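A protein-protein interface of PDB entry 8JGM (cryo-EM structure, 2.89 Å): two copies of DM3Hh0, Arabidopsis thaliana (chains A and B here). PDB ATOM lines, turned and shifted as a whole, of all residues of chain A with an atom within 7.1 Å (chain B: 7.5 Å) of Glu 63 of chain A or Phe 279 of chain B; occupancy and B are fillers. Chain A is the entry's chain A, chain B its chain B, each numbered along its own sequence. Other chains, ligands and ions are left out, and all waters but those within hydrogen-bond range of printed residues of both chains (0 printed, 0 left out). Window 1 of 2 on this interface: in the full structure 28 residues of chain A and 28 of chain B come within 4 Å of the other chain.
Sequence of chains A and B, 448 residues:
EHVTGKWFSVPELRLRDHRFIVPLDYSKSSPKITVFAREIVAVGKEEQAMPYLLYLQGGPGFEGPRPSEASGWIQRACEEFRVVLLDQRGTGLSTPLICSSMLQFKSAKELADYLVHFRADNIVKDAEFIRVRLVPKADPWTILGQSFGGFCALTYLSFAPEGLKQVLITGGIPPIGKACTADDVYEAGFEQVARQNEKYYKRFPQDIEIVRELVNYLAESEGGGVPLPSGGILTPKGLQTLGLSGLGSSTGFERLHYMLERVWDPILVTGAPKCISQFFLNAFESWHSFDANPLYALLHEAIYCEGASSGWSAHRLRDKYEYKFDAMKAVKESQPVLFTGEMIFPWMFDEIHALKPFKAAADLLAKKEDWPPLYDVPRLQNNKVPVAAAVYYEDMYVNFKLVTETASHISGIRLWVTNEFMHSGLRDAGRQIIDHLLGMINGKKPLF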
ATOM      1  N   TYR A  55     -35.491  21.092 -23.491  1.00  0.00           N
ATOM      2  CA  TYR A  55     -35.182  22.518 -23.396  1.00  0.00           C
ATOM      3  C   TYR A  55     -33.697  22.796 -23.639  1.00  0.00           C
ATOM      4  O   TYR A  55     -32.846  22.175 -23.010  1.00  0.00           O
ATOM      5  CB  TYR A  55     -35.600  23.012 -22.018  1.00  0.00           C
ATOM      6  CG  TYR A  55     -35.432  24.502 -21.838  1.00  0.00           C
ATOM      7  CD1 TYR A  55     -36.375  25.369 -22.406  1.00  0.00           C
ATOM      8  CD2 TYR A  55     -34.348  25.022 -21.114  1.00  0.00           C
ATOM      9  CE1 TYR A  55     -36.253  26.755 -22.244  1.00  0.00           C
ATOM     10  CE2 TYR A  55     -34.222  26.412 -20.947  1.00  0.00           C
ATOM     11  CZ  TYR A  55     -35.178  27.281 -21.507  1.00  0.00           C
ATOM     12  OH  TYR A  55     -35.070  28.619 -21.328  1.00  0.00           O
ATOM     13  N   GLN A  57     -30.787  25.796 -23.417  1.00  0.00           N
ATOM     14  CA  GLN A  57     -30.635  27.004 -22.603  1.00  0.00           C
ATOM     15  C   GLN A  57     -30.051  28.199 -23.367  1.00  0.00           C
ATOM     16  O   GLN A  57     -29.246  28.066 -24.284  1.00  0.00           O
ATOM     17  CB  GLN A  57     -29.821  26.640 -21.352  1.00  0.00           C
ATOM     18  CG  GLN A  57     -29.449  27.779 -20.393  1.00  0.00           C
ATOM     19  CD  GLN A  57     -30.641  28.478 -19.746  1.00  0.00           C
ATOM     20  OE1 GLN A  57     -31.547  28.952 -20.406  1.00  0.00           O
ATOM     21  NE2 GLN A  57     -30.671  28.606 -18.442  1.00  0.00           N
ATOM     22  N   GLY A  58     -30.434  29.403 -22.947  1.00  0.00           N
ATOM     23  CA  GLY A  58     -30.138  30.677 -23.600  1.00  0.00           C
ATOM     24  C   GLY A  58     -28.744  31.261 -23.370  1.00  0.00           C
ATOM     25  O   GLY A  58     -28.633  32.443 -23.050  1.00  0.00           O
ATOM     26  N   GLY A  59     -27.680  30.490 -23.564  1.00  0.00           N
ATOM     27  CA  GLY A  59     -26.340  31.067 -23.694  1.00  0.00           C
ATOM     28  C   GLY A  59     -25.226  30.043 -23.910  1.00  0.00           C
ATOM     29  O   GLY A  59     -25.438  28.855 -23.660  1.00  0.00           O
ATOM     30  N   GLY A  61     -22.627  29.199 -22.202  1.00  0.00           N
ATOM     31  CA  GLY A  61     -22.024  28.590 -21.008  1.00  0.00           C
ATOM     32  C   GLY A  61     -22.874  28.564 -19.739  1.00  0.00           C
ATOM     33  O   GLY A  61     -22.318  28.332 -18.667  1.00  0.00           O
ATOM     34  N   PHE A  62     -24.186  28.802 -19.799  1.00  0.00           N
ATOM     35  CA  PHE A  62     -25.053  28.839 -18.612  1.00  0.00           C
ATOM     36  C   PHE A  62     -25.667  27.478 -18.249  1.00  0.00           C
ATOM     37  O   PHE A  62     -26.046  26.701 -19.121  1.00  0.00           O
ATOM     38  CB  PHE A  62     -26.161  29.880 -18.800  1.00  0.00           C
ATOM     39  CG  PHE A  62     -25.691  31.296 -19.069  1.00  0.00           C
ATOM     40  CD1 PHE A  62     -24.641  31.862 -18.326  1.00  0.00           C
ATOM     41  CD2 PHE A  62     -26.328  32.067 -20.055  1.00  0.00           C
ATOM     42  CE1 PHE A  62     -24.208  33.171 -18.591  1.00  0.00           C
ATOM     43  CE2 PHE A  62     -25.898  33.378 -20.317  1.00  0.00           C
ATOM     44  CZ  PHE A  62     -24.832  33.926 -19.592  1.00  0.00           C
ATOM     45  N   GLU A  63     -25.818  27.218 -16.951  1.00  0.00           N
ATOM     46  CA  GLU A  63     -26.592  26.093 -16.416  1.00  0.00           C
ATOM     47  C   GLU A  63     -28.082  26.174 -16.776  1.00  0.00           C
ATOM     48  O   GLU A  63     -28.591  27.253 -17.079  1.00  0.00           O
ATOM     49  CB  GLU A  63     -26.462  26.059 -14.885  1.00  0.00           C
ATOM     50  CG  GLU A  63     -25.022  25.858 -14.397  1.00  0.00           C
ATOM     51  CD  GLU A  63     -24.316  27.143 -13.932  1.00  0.00           C
ATOM     52  OE1 GLU A  63     -24.376  28.170 -14.649  1.00  0.00           O
ATOM     53  OE2 GLU A  63     -23.685  27.095 -12.849  1.00  0.00           O
ATOM     54  N   GLY A  64     -28.803  25.051 -16.707  1.00  0.00           N
ATOM     55  CA  GLY A  64     -30.253  25.009 -16.921  1.00  0.00           C
ATOM     56  C   GLY A  64     -31.086  25.769 -15.868  1.00  0.00           C
ATOM     57  O   GLY A  64     -30.537  26.357 -14.941  1.00  0.00           O
ATOM     58  N   PRO A  65     -32.426  25.770 -15.980  1.00  0.00           N
ATOM     59  CA  PRO A  65     -33.304  26.623 -15.171  1.00  0.00           C
ATOM     60  C   PRO A  65     -33.280  26.449 -13.644  1.00  0.00           C
ATOM     61  O   PRO A  65     -33.533  27.423 -12.940  1.00  0.00           O
ATOM     62  CB  PRO A  65     -34.710  26.357 -15.705  1.00  0.00           C
ATOM     63  CG  PRO A  65     -34.458  26.047 -17.173  1.00  0.00           C
ATOM     64  CD  PRO A  65     -33.151  25.268 -17.133  1.00  0.00           C
ATOM     65  N   ARG A  66     -33.021  25.245 -13.112  1.00  0.00           N
ATOM     66  CA  ARG A  66     -33.022  24.939 -11.656  1.00  0.00           C
ATOM     67  C   ARG A  66     -34.279  25.461 -10.919  1.00  0.00           C
ATOM     68  O   ARG A  66     -34.176  26.365 -10.088  1.00  0.00           O
ATOM     69  CB  ARG A  66     -31.724  25.455 -10.998  1.00  0.00           C
ATOM     70  CG  ARG A  66     -30.424  24.959 -11.640  1.00  0.00           C
ATOM     71  CD  ARG A  66     -30.288  23.433 -11.626  1.00  0.00           C
ATOM     72  NE  ARG A  66     -29.100  22.982 -12.378  1.00  0.00           N
ATOM     73  CZ  ARG A  66     -27.843  23.136 -12.027  1.00  0.00           C
ATOM     74  NH1 ARG A  66     -26.875  22.724 -12.789  1.00  0.00           N
ATOM     75  NH2 ARG A  66     -27.510  23.700 -10.908  1.00  0.00           N
ATOM     76  N   LEU A  86     -31.518  20.191 -19.676  1.00  0.00           N
ATOM     77  CA  LEU A  86     -30.244  19.519 -19.892  1.00  0.00           C
ATOM     78  C   LEU A  86     -29.038  20.451 -19.833  1.00  0.00           C
ATOM     79  O   LEU A  86     -28.939  21.404 -20.603  1.00  0.00           O
ATOM     80  CB  LEU A  86     -30.268  18.773 -21.231  1.00  0.00           C
ATOM     81  CG  LEU A  86     -29.096  17.848 -21.566  1.00  0.00           C
ATOM     82  CD1 LEU A  86     -29.573  16.661 -22.390  1.00  0.00           C
ATOM     83  CD2 LEU A  86     -28.008  18.612 -22.302  1.00  0.00           C
ATOM     84  N   ASP A  87     -28.121  20.160 -18.915  1.00  0.00           N
ATOM     85  CA  ASP A  87     -26.899  20.954 -18.766  1.00  0.00           C
ATOM     86  C   ASP A  87     -25.979  20.642 -19.948  1.00  0.00           C
ATOM     87  O   ASP A  87     -25.497  19.521 -20.094  1.00  0.00           O
ATOM     88  CB  ASP A  87     -26.196  20.682 -17.422  1.00  0.00           C
ATOM     89  CG  ASP A  87     -26.721  21.509 -16.240  1.00  0.00           C
ATOM     90  OD1 ASP A  87     -27.538  22.434 -16.435  1.00  0.00           O
ATOM     91  OD2 ASP A  87     -26.255  21.269 -15.100  1.00  0.00           O
ATOM     92  N   GLN A  88     -25.742  21.625 -20.812  1.00  0.00           N
ATOM     93  CA  GLN A  88     -24.871  21.471 -21.979  1.00  0.00           C
ATOM     94  C   GLN A  88     -23.423  21.191 -21.555  1.00  0.00           C
ATOM     95  O   GLN A  88     -22.981  21.644 -20.501  1.00  0.00           O
ATOM     96  CB  GLN A  88     -24.978  22.731 -22.846  1.00  0.00           C
ATOM     97  CG  GLN A  88     -26.348  22.810 -23.551  1.00  0.00           C
ATOM     98  CD  GLN A  88     -26.909  24.220 -23.735  1.00  0.00           C
ATOM     99  OE1 GLN A  88     -28.114  24.428 -23.719  1.00  0.00           O
ATOM    100  NE2 GLN A  88     -26.093  25.236 -23.894  1.00  0.00           N
ATOM    101  N   THR A  91     -20.565  23.052 -18.790  1.00  0.00           N
ATOM    102  CA  THR A  91     -21.217  23.880 -17.764  1.00  0.00           C
ATOM    103  C   THR A  91     -22.109  23.071 -16.822  1.00  0.00           C
ATOM    104  O   THR A  91     -22.481  21.937 -17.110  1.00  0.00           O
ATOM    105  CB  THR A  91     -21.954  25.055 -18.415  1.00  0.00           C
ATOM    106  OG1 THR A  91     -22.422  25.926 -17.419  1.00  0.00           O
ATOM    107  CG2 THR A  91     -23.150  24.668 -19.275  1.00  0.00           C
ATOM    108  N   GLY A  92     -22.427  23.630 -15.653  1.00  0.00           N
ATOM    109  CA  GLY A  92     -23.287  22.998 -14.656  1.00  0.00           C
ATOM    110  C   GLY A  92     -22.712  21.697 -14.125  1.00  0.00           C
ATOM    111  O   GLY A  92     -21.531  21.639 -13.795  1.00  0.00           O
ATOM    112  N   LEU A  93     -23.518  20.645 -14.032  1.00  0.00           N
ATOM    113  CA  LEU A  93     -23.015  19.323 -13.649  1.00  0.00           C
ATOM    114  C   LEU A  93     -22.339  18.588 -14.821  1.00  0.00           C
ATOM    115  O   LEU A  93     -21.645  17.599 -14.603  1.00  0.00           O
ATOM    116  CB  LEU A  93     -24.153  18.498 -13.028  1.00  0.00           C
ATOM    117  CG  LEU A  93     -24.359  18.769 -11.527  1.00  0.00           C
ATOM    118  CD1 LEU A  93     -24.856  20.176 -11.221  1.00  0.00           C
ATOM    119  CD2 LEU A  93     -25.388  17.805 -10.956  1.00  0.00           C
ATOM    120  N   CYS A  99     -10.755  23.761 -11.126  1.00  0.00           N
ATOM    121  CA  CYS A  99     -10.116  24.848 -10.374  1.00  0.00           C
ATOM    122  C   CYS A  99      -9.860  24.442  -8.900  1.00  0.00           C
ATOM    123  O   CYS A  99     -10.363  23.422  -8.433  1.00  0.00           O
ATOM    124  CB  CYS A  99     -10.988  26.106 -10.524  1.00  0.00           C
ATOM    125  SG  CYS A  99     -10.087  27.604 -10.040  1.00  0.00           S
ATOM    126  N   ASP A 291     -17.097  35.296 -13.512  1.00  0.00           N
ATOM    127  CA  ASP A 291     -16.533  34.469 -12.446  1.00  0.00           C
ATOM    128  C   ASP A 291     -17.124  33.054 -12.413  1.00  0.00           C
ATOM    129  O   ASP A 291     -16.391  32.082 -12.238  1.00  0.00           O
ATOM    130  CB  ASP A 291     -16.757  35.154 -11.082  1.00  0.00           C
ATOM    131  CG  ASP A 291     -18.216  35.513 -10.738  1.00  0.00           C
ATOM    132  OD1 ASP A 291     -19.080  35.559 -11.641  1.00  0.00           O
ATOM    133  OD2 ASP A 291     -18.490  35.750  -9.538  1.00  0.00           O
ATOM    134  N   ALA A 292     -18.438  32.920 -12.570  1.00  0.00           N
ATOM    135  CA  ALA A 292     -19.141  31.645 -12.499  1.00  0.00           C
ATOM    136  C   ALA A 292     -19.205  30.910 -13.849  1.00  0.00           C
ATOM    137  O   ALA A 292     -19.232  29.680 -13.872  1.00  0.00           O
ATOM    138  CB  ALA A 292     -20.543  31.922 -11.956  1.00  0.00           C
ATOM    139  N   ASN A 293     -19.233  31.639 -14.967  1.00  0.00           N
ATOM    140  CA  ASN A 293     -19.459  31.091 -16.305  1.00  0.00           C
ATOM    141  C   ASN A 293     -18.389  31.570 -17.308  1.00  0.00           C
ATOM    142  O   ASN A 293     -18.728  32.194 -18.312  1.00  0.00           O
ATOM    143  CB  ASN A 293     -20.899  31.430 -16.734  1.00  0.00           C
ATOM    144  CG  ASN A 293     -21.940  30.840 -15.802  1.00  0.00           C
ATOM    145  OD1 ASN A 293     -22.345  31.447 -14.825  1.00  0.00           O
ATOM    146  ND2 ASN A 293     -22.414  29.650 -16.084  1.00  0.00           N
ATOM    147  N   TYR B 258     -29.815  22.322  -4.140  1.00  0.00           N
ATOM    148  CA  TYR B 258     -29.100  22.558  -5.397  1.00  0.00           C
ATOM    149  C   TYR B 258     -27.677  23.084  -5.197  1.00  0.00           C
ATOM    150  O   TYR B 258     -26.841  22.885  -6.071  1.00  0.00           O
ATOM    151  CB  TYR B 258     -29.871  23.544  -6.276  1.00  0.00           C
ATOM    152  CG  TYR B 258     -31.203  23.055  -6.799  1.00  0.00           C
ATOM    153  CD1 TYR B 258     -31.306  21.794  -7.414  1.00  0.00           C
ATOM    154  CD2 TYR B 258     -32.322  23.897  -6.740  1.00  0.00           C
ATOM    155  CE1 TYR B 258     -32.535  21.369  -7.947  1.00  0.00           C
ATOM    156  CE2 TYR B 258     -33.549  23.482  -7.283  1.00  0.00           C
ATOM    157  CZ  TYR B 258     -33.655  22.215  -7.883  1.00  0.00           C
ATOM    158  OH  TYR B 258     -34.826  21.816  -8.431  1.00  0.00           O
ATOM    159  N   MET B 259     -27.362  23.734  -4.080  1.00  0.00           N
ATOM    160  CA  MET B 259     -26.001  24.182  -3.799  1.00  0.00           C
ATOM    161  C   MET B 259     -25.090  23.024  -3.397  1.00  0.00           C
ATOM    162  O   MET B 259     -23.966  22.932  -3.883  1.00  0.00           O
ATOM    163  CB  MET B 259     -26.046  25.263  -2.725  1.00  0.00           C
ATOM    164  CG  MET B 259     -24.673  25.841  -2.406  1.00  0.00           C
ATOM    165  SD  MET B 259     -24.809  27.269  -1.311  1.00  0.00           S
ATOM    166  CE  MET B 259     -23.072  27.659  -1.030  1.00  0.00           C
ATOM    167  N   GLU B 261     -25.142  19.951  -4.353  1.00  0.00           N
ATOM    168  CA  GLU B 261     -24.731  19.142  -5.511  1.00  0.00           C
ATOM    169  C   GLU B 261     -23.352  19.548  -6.069  1.00  0.00           C
ATOM    170  O   GLU B 261     -22.680  18.729  -6.694  1.00  0.00           O
ATOM    171  CB  GLU B 261     -25.766  19.259  -6.640  1.00  0.00           C
ATOM    172  CG  GLU B 261     -27.107  18.583  -6.325  1.00  0.00           C
ATOM    173  CD  GLU B 261     -28.102  18.666  -7.500  1.00  0.00           C
ATOM    174  OE1 GLU B 261     -28.035  19.616  -8.306  1.00  0.00           O
ATOM    175  OE2 GLU B 261     -28.987  17.787  -7.633  1.00  0.00           O
ATOM    176  N   ARG B 262     -23.015  20.829  -5.939  1.00  0.00           N
ATOM    177  CA  ARG B 262     -21.794  21.368  -6.533  1.00  0.00           C
ATOM    178  C   ARG B 262     -20.599  21.623  -5.628  1.00  0.00           C
ATOM    179  O   ARG B 262     -19.909  22.633  -5.772  1.00  0.00           O
ATOM    180  CB  ARG B 262     -22.121  22.642  -7.324  1.00  0.00           C
ATOM    181  CG  ARG B 262     -23.539  22.686  -7.871  1.00  0.00           C
ATOM    182  CD  ARG B 262     -23.550  22.545  -9.385  1.00  0.00           C
ATOM    183  NE  ARG B 262     -22.576  23.426 -10.024  1.00  0.00           N
ATOM    184  CZ  ARG B 262     -22.886  24.573 -10.619  1.00  0.00           C
ATOM    185  NH1 ARG B 262     -21.935  25.312 -11.174  1.00  0.00           N
ATOM    186  NH2 ARG B 262     -24.147  24.982 -10.659  1.00  0.00           N
ATOM    187  N   VAL B 263     -20.340  20.708  -4.708  1.00  0.00           N
ATOM    188  CA  VAL B 263     -19.168  20.865  -3.827  1.00  0.00           C
ATOM    189  C   VAL B 263     -17.847  20.365  -4.409  1.00  0.00           C
ATOM    190  O   VAL B 263     -16.842  21.040  -4.228  1.00  0.00           O
ATOM    191  CB  VAL B 263     -19.381  20.231  -2.446  1.00  0.00           C
ATOM    192  CG1 VAL B 263     -20.356  21.068  -1.627  1.00  0.00           C
ATOM    193  CG2 VAL B 263     -19.900  18.799  -2.495  1.00  0.00           C
ATOM    194  N   ASP B 265     -14.921  19.420  -7.119  1.00  0.00           N
ATOM    195  CA  ASP B 265     -14.304  19.688  -8.413  1.00  0.00           C
ATOM    196  C   ASP B 265     -14.206  18.379  -9.235  1.00  0.00           C
ATOM    197  O   ASP B 265     -13.767  17.364  -8.688  1.00  0.00           O
ATOM    198  CB  ASP B 265     -12.932  20.289  -8.087  1.00  0.00           C
ATOM    199  CG  ASP B 265     -12.148  20.730  -9.315  1.00  0.00           C
ATOM    200  OD1 ASP B 265     -12.609  21.666 -10.004  1.00  0.00           O
ATOM    201  OD2 ASP B 265     -11.081  20.125  -9.553  1.00  0.00           O
ATOM    202  N   ILE B 276     -12.470  21.138  -3.187  1.00  0.00           N
ATOM    203  CA  ILE B 276     -13.694  21.926  -3.200  1.00  0.00           C
ATOM    204  C   ILE B 276     -13.744  22.767  -4.486  1.00  0.00           C
ATOM    205  O   ILE B 276     -12.727  23.311  -4.911  1.00  0.00           O
ATOM    206  CB  ILE B 276     -13.765  22.751  -1.900  1.00  0.00           C
ATOM    207  CG1 ILE B 276     -15.170  23.311  -1.647  1.00  0.00           C
ATOM    208  CG2 ILE B 276     -12.748  23.898  -1.868  1.00  0.00           C
ATOM    209  CD1 ILE B 276     -16.084  22.232  -1.062  1.00  0.00           C
ATOM    210  N   SER B 277     -14.894  22.849  -5.147  1.00  0.00           N
ATOM    211  CA  SER B 277     -15.023  23.562  -6.420  1.00  0.00           C
ATOM    212  C   SER B 277     -14.961  25.079  -6.237  1.00  0.00           C
ATOM    213  O   SER B 277     -15.431  25.631  -5.240  1.00  0.00           O
ATOM    214  CB  SER B 277     -16.296  23.151  -7.162  1.00  0.00           C
ATOM    215  OG  SER B 277     -17.445  23.759  -6.613  1.00  0.00           O
ATOM    216  N   GLN B 278     -14.433  25.788  -7.234  1.00  0.00           N
ATOM    217  CA  GLN B 278     -14.400  27.251  -7.209  1.00  0.00           C
ATOM    218  C   GLN B 278     -15.812  27.838  -7.177  1.00  0.00           C
ATOM    219  O   GLN B 278     -16.051  28.819  -6.480  1.00  0.00           O
ATOM    220  CB  GLN B 278     -13.596  27.750  -8.417  1.00  0.00           C
ATOM    221  CG  GLN B 278     -13.473  29.278  -8.524  1.00  0.00           C
ATOM    222  CD  GLN B 278     -12.684  29.922  -7.386  1.00  0.00           C
ATOM    223  OE1 GLN B 278     -12.000  29.282  -6.602  1.00  0.00           O
ATOM    224  NE2 GLN B 278     -12.733  31.226  -7.262  1.00  0.00           N
ATOM    225  N   PHE B 279     -16.767  27.202  -7.857  1.00  0.00           N
ATOM    226  CA  PHE B 279     -18.170  27.581  -7.779  1.00  0.00           C
ATOM    227  C   PHE B 279     -18.694  27.507  -6.346  1.00  0.00           C
ATOM    228  O   PHE B 279     -19.321  28.462  -5.904  1.00  0.00           O
ATOM    229  CB  PHE B 279     -19.011  26.711  -8.710  1.00  0.00           C
ATOM    230  CG  PHE B 279     -20.486  27.065  -8.675  1.00  0.00           C
ATOM    231  CD1 PHE B 279     -21.000  28.016  -9.570  1.00  0.00           C
ATOM    232  CD2 PHE B 279     -21.329  26.484  -7.715  1.00  0.00           C
ATOM    233  CE1 PHE B 279     -22.357  28.383  -9.505  1.00  0.00           C
ATOM    234  CE2 PHE B 279     -22.681  26.864  -7.637  1.00  0.00           C
ATOM    235  CZ  PHE B 279     -23.192  27.813  -8.533  1.00  0.00           C
ATOM    236  N   PHE B 280     -18.427  26.435  -5.587  1.00  0.00           N
ATOM    237  CA  PHE B 280     -18.955  26.374  -4.228  1.00  0.00           C
ATOM    238  C   PHE B 280     -18.356  27.461  -3.340  1.00  0.00           C
ATOM    239  O   PHE B 280     -19.097  28.140  -2.637  1.00  0.00           O
ATOM    240  CB  PHE B 280     -18.732  24.990  -3.629  1.00  0.00           C
ATOM    241  CG  PHE B 280     -19.289  24.876  -2.229  1.00  0.00           C
ATOM    242  CD1 PHE B 280     -20.655  24.627  -2.036  1.00  0.00           C
ATOM    243  CD2 PHE B 280     -18.448  25.054  -1.120  1.00  0.00           C
ATOM    244  CE1 PHE B 280     -21.175  24.530  -0.735  1.00  0.00           C
ATOM    245  CE2 PHE B 280     -18.969  24.973   0.180  1.00  0.00           C
ATOM    246  CZ  PHE B 280     -20.333  24.707   0.373  1.00  0.00           C
ATOM    247  N   LEU B 281     -17.044  27.708  -3.400  1.00  0.00           N
ATOM    248  CA  LEU B 281     -16.445  28.786  -2.606  1.00  0.00           C
ATOM    249  C   LEU B 281     -17.001  30.154  -2.995  1.00  0.00           C
ATOM    250  O   LEU B 281     -17.318  30.965  -2.129  1.00  0.00           O
ATOM    251  CB  LEU B 281     -14.920  28.784  -2.755  1.00  0.00           C
ATOM    252  CG  LEU B 281     -14.222  27.537  -2.202  1.00  0.00           C
ATOM    253  CD1 LEU B 281     -12.716  27.708  -2.379  1.00  0.00           C
ATOM    254  CD2 LEU B 281     -14.504  27.329  -0.715  1.00  0.00           C
ATOM    255  N   ASN B 282     -17.171  30.406  -4.289  1.00  0.00           N
ATOM    256  CA  ASN B 282     -17.727  31.666  -4.756  1.00  0.00           C
ATOM    257  C   ASN B 282     -19.198  31.851  -4.339  1.00  0.00           C
ATOM    258  O   ASN B 282     -19.608  32.937  -3.932  1.00  0.00           O
ATOM    259  CB  ASN B 282     -17.557  31.687  -6.277  1.00  0.00           C
ATOM    260  CG  ASN B 282     -17.828  33.055  -6.853  1.00  0.00           C
ATOM    261  OD1 ASN B 282     -17.408  34.063  -6.316  1.00  0.00           O
ATOM    262  ND2 ASN B 282     -18.520  33.133  -7.958  1.00  0.00           N
ATOM    263  N   ALA B 283     -20.000  30.791  -4.399  1.00  0.00           N
ATOM    264  CA  ALA B 283     -21.385  30.818  -3.951  1.00  0.00           C
ATOM    265  C   ALA B 283     -21.481  31.045  -2.438  1.00  0.00           C
ATOM    266  O   ALA B 283     -22.233  31.909  -2.007  1.00  0.00           O
ATOM    267  CB  ALA B 283     -22.061  29.511  -4.360  1.00  0.00           C
ATOM    268  N   PHE B 284     -20.689  30.333  -1.634  1.00  0.00           N
ATOM    269  CA  PHE B 284     -20.664  30.513  -0.184  1.00  0.00           C
ATOM    270  C   PHE B 284     -20.269  31.938   0.207  1.00  0.00           C
ATOM    271  O   PHE B 284     -20.943  32.567   1.014  1.00  0.00           O
ATOM    272  CB  PHE B 284     -19.708  29.490   0.428  1.00  0.00           C
ATOM    273  CG  PHE B 284     -19.583  29.614   1.930  1.00  0.00           C
ATOM    274  CD1 PHE B 284     -20.444  28.893   2.769  1.00  0.00           C
ATOM    275  CD2 PHE B 284     -18.624  30.472   2.488  1.00  0.00           C
ATOM    276  CE1 PHE B 284     -20.357  29.044   4.164  1.00  0.00           C
ATOM    277  CE2 PHE B 284     -18.539  30.631   3.881  1.00  0.00           C
ATOM    278  CZ  PHE B 284     -19.414  29.918   4.720  1.00  0.00           C
ATOM    279  N   GLU B 285     -19.229  32.495  -0.409  1.00  0.00           N
ATOM    280  CA  GLU B 285     -18.840  33.892  -0.213  1.00  0.00           C
ATOM    281  C   GLU B 285     -19.985  34.871  -0.530  1.00  0.00           C
ATOM    282  O   GLU B 285     -20.112  35.912   0.106  1.00  0.00           O
ATOM    283  CB  GLU B 285     -17.612  34.166  -1.092  1.00  0.00           C
ATOM    284  CG  GLU B 285     -17.110  35.606  -0.998  1.00  0.00           C
ATOM    285  CD  GLU B 285     -15.818  35.789  -1.805  1.00  0.00           C
ATOM    286  OE1 GLU B 285     -14.751  35.340  -1.338  1.00  0.00           O
ATOM    287  OE2 GLU B 285     -15.883  36.421  -2.883  1.00  0.00           O
ATOM    288  N   SER B 286     -20.842  34.535  -1.491  1.00  0.00           N
ATOM    289  CA  SER B 286     -21.976  35.356  -1.925  1.00  0.00           C
ATOM    290  C   SER B 286     -23.269  35.141  -1.127  1.00  0.00           C
ATOM    291  O   SER B 286     -24.254  35.832  -1.377  1.00  0.00           O
ATOM    292  CB  SER B 286     -22.268  35.061  -3.397  1.00  0.00           C
ATOM    293  OG  SER B 286     -21.098  35.188  -4.183  1.00  0.00           O
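The side-chain carboxylate of Asp 265 of chain B lies within hydrogen-bond range of the backbone NH of Cys 99 of chain A, at 3.0 Å.
ND2 of Asn 282 of chain B is in hydrogen-bond range of OD2 of Asp 291 of chain A (3.1 Å).
NH1 of Arg 262 of chain B is in salt-bridge range of OE2 of Glu 63 of chain A, 3.0 Å away.
The side-chain amide nitrogen of Asn 293 of chain A is in hydrogen-bond range of the side-chain carboxylate of Glu 63 of chain A (2.8 Å).
The side-chain carboxylate (OD2) of Asp 87 of chain A is in salt-bridge range of the guanidinium group (NH1) of Arg 66 of chain A (2.8 Å).
N of Leu 93 of chain A lies within hydrogen-bond range of OD2 of Asp 87 of chain A (3.0 Å).
The backbone carbonyl oxygen (O) of Asn 282 of chain B lies within hydrogen-bond range of the side-chain hydroxyl (OG) of Ser 286 of chain B (2.7 Å).
The side-chain hydroxyl (OG) of Ser 277 of chain B sits at hydrogen-bond distance from the backbone carbonyl oxygen (O) of Arg 262 of chain B, at 2.8 Å.
The side-chain amide nitrogen (NE2) of Gln 57 of chain A lies within hydrogen-bond range of the backbone carbonyl oxygen (O) of Glu 63 of chain A (2.8 Å).
Phe 279 of chain B touches Glu 63 of chain A.
Arg 66 of chain A touches Arg 262 of chain B.
Arg 262 of chain B touches Leu 93 of chain A (CD to CD1, 3.3 Å).
Gln 278 of chain B touches Cys 99 of chain A.
Printed residues of chain B within 4 Å of Arg 66 of chain A: Arg 262.
Of the printed residues of chain A, Asp 265 of chain B touches Cys 99.
Printed residues of chain A within 4 Å of Gln 278 of chain B: Cys 99.
Phe 279 of chain B touches one residue of chain A.
Of the printed residues of chain A, Asn 282 of chain B touches Asp 291.
The nearest printed residue of chain B that does not touch Arg 66 of chain A is Tyr 258 of chain B (4.1 Å).
Of the 20 printed residues of chain A, 5 touch a printed residue of chain B.
Of the 17 printed residues of chain B, 5 touch a printed residue of chain A.
Hydrophobic or aromatic side chains of chain B within 4 Å of the printed part of chain A: Phe 279.
Along chain B the printed residues that touch a printed residue of chain A span positions 262 to 282.
Among the printed residues, Asp or Glu carboxylates within 4 Å of a Lys or Arg side-chain nitrogen of the other chain: Glu 63 of chain A with Arg 262 of chain B (3.0 Å).
No position is printed for both chains.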
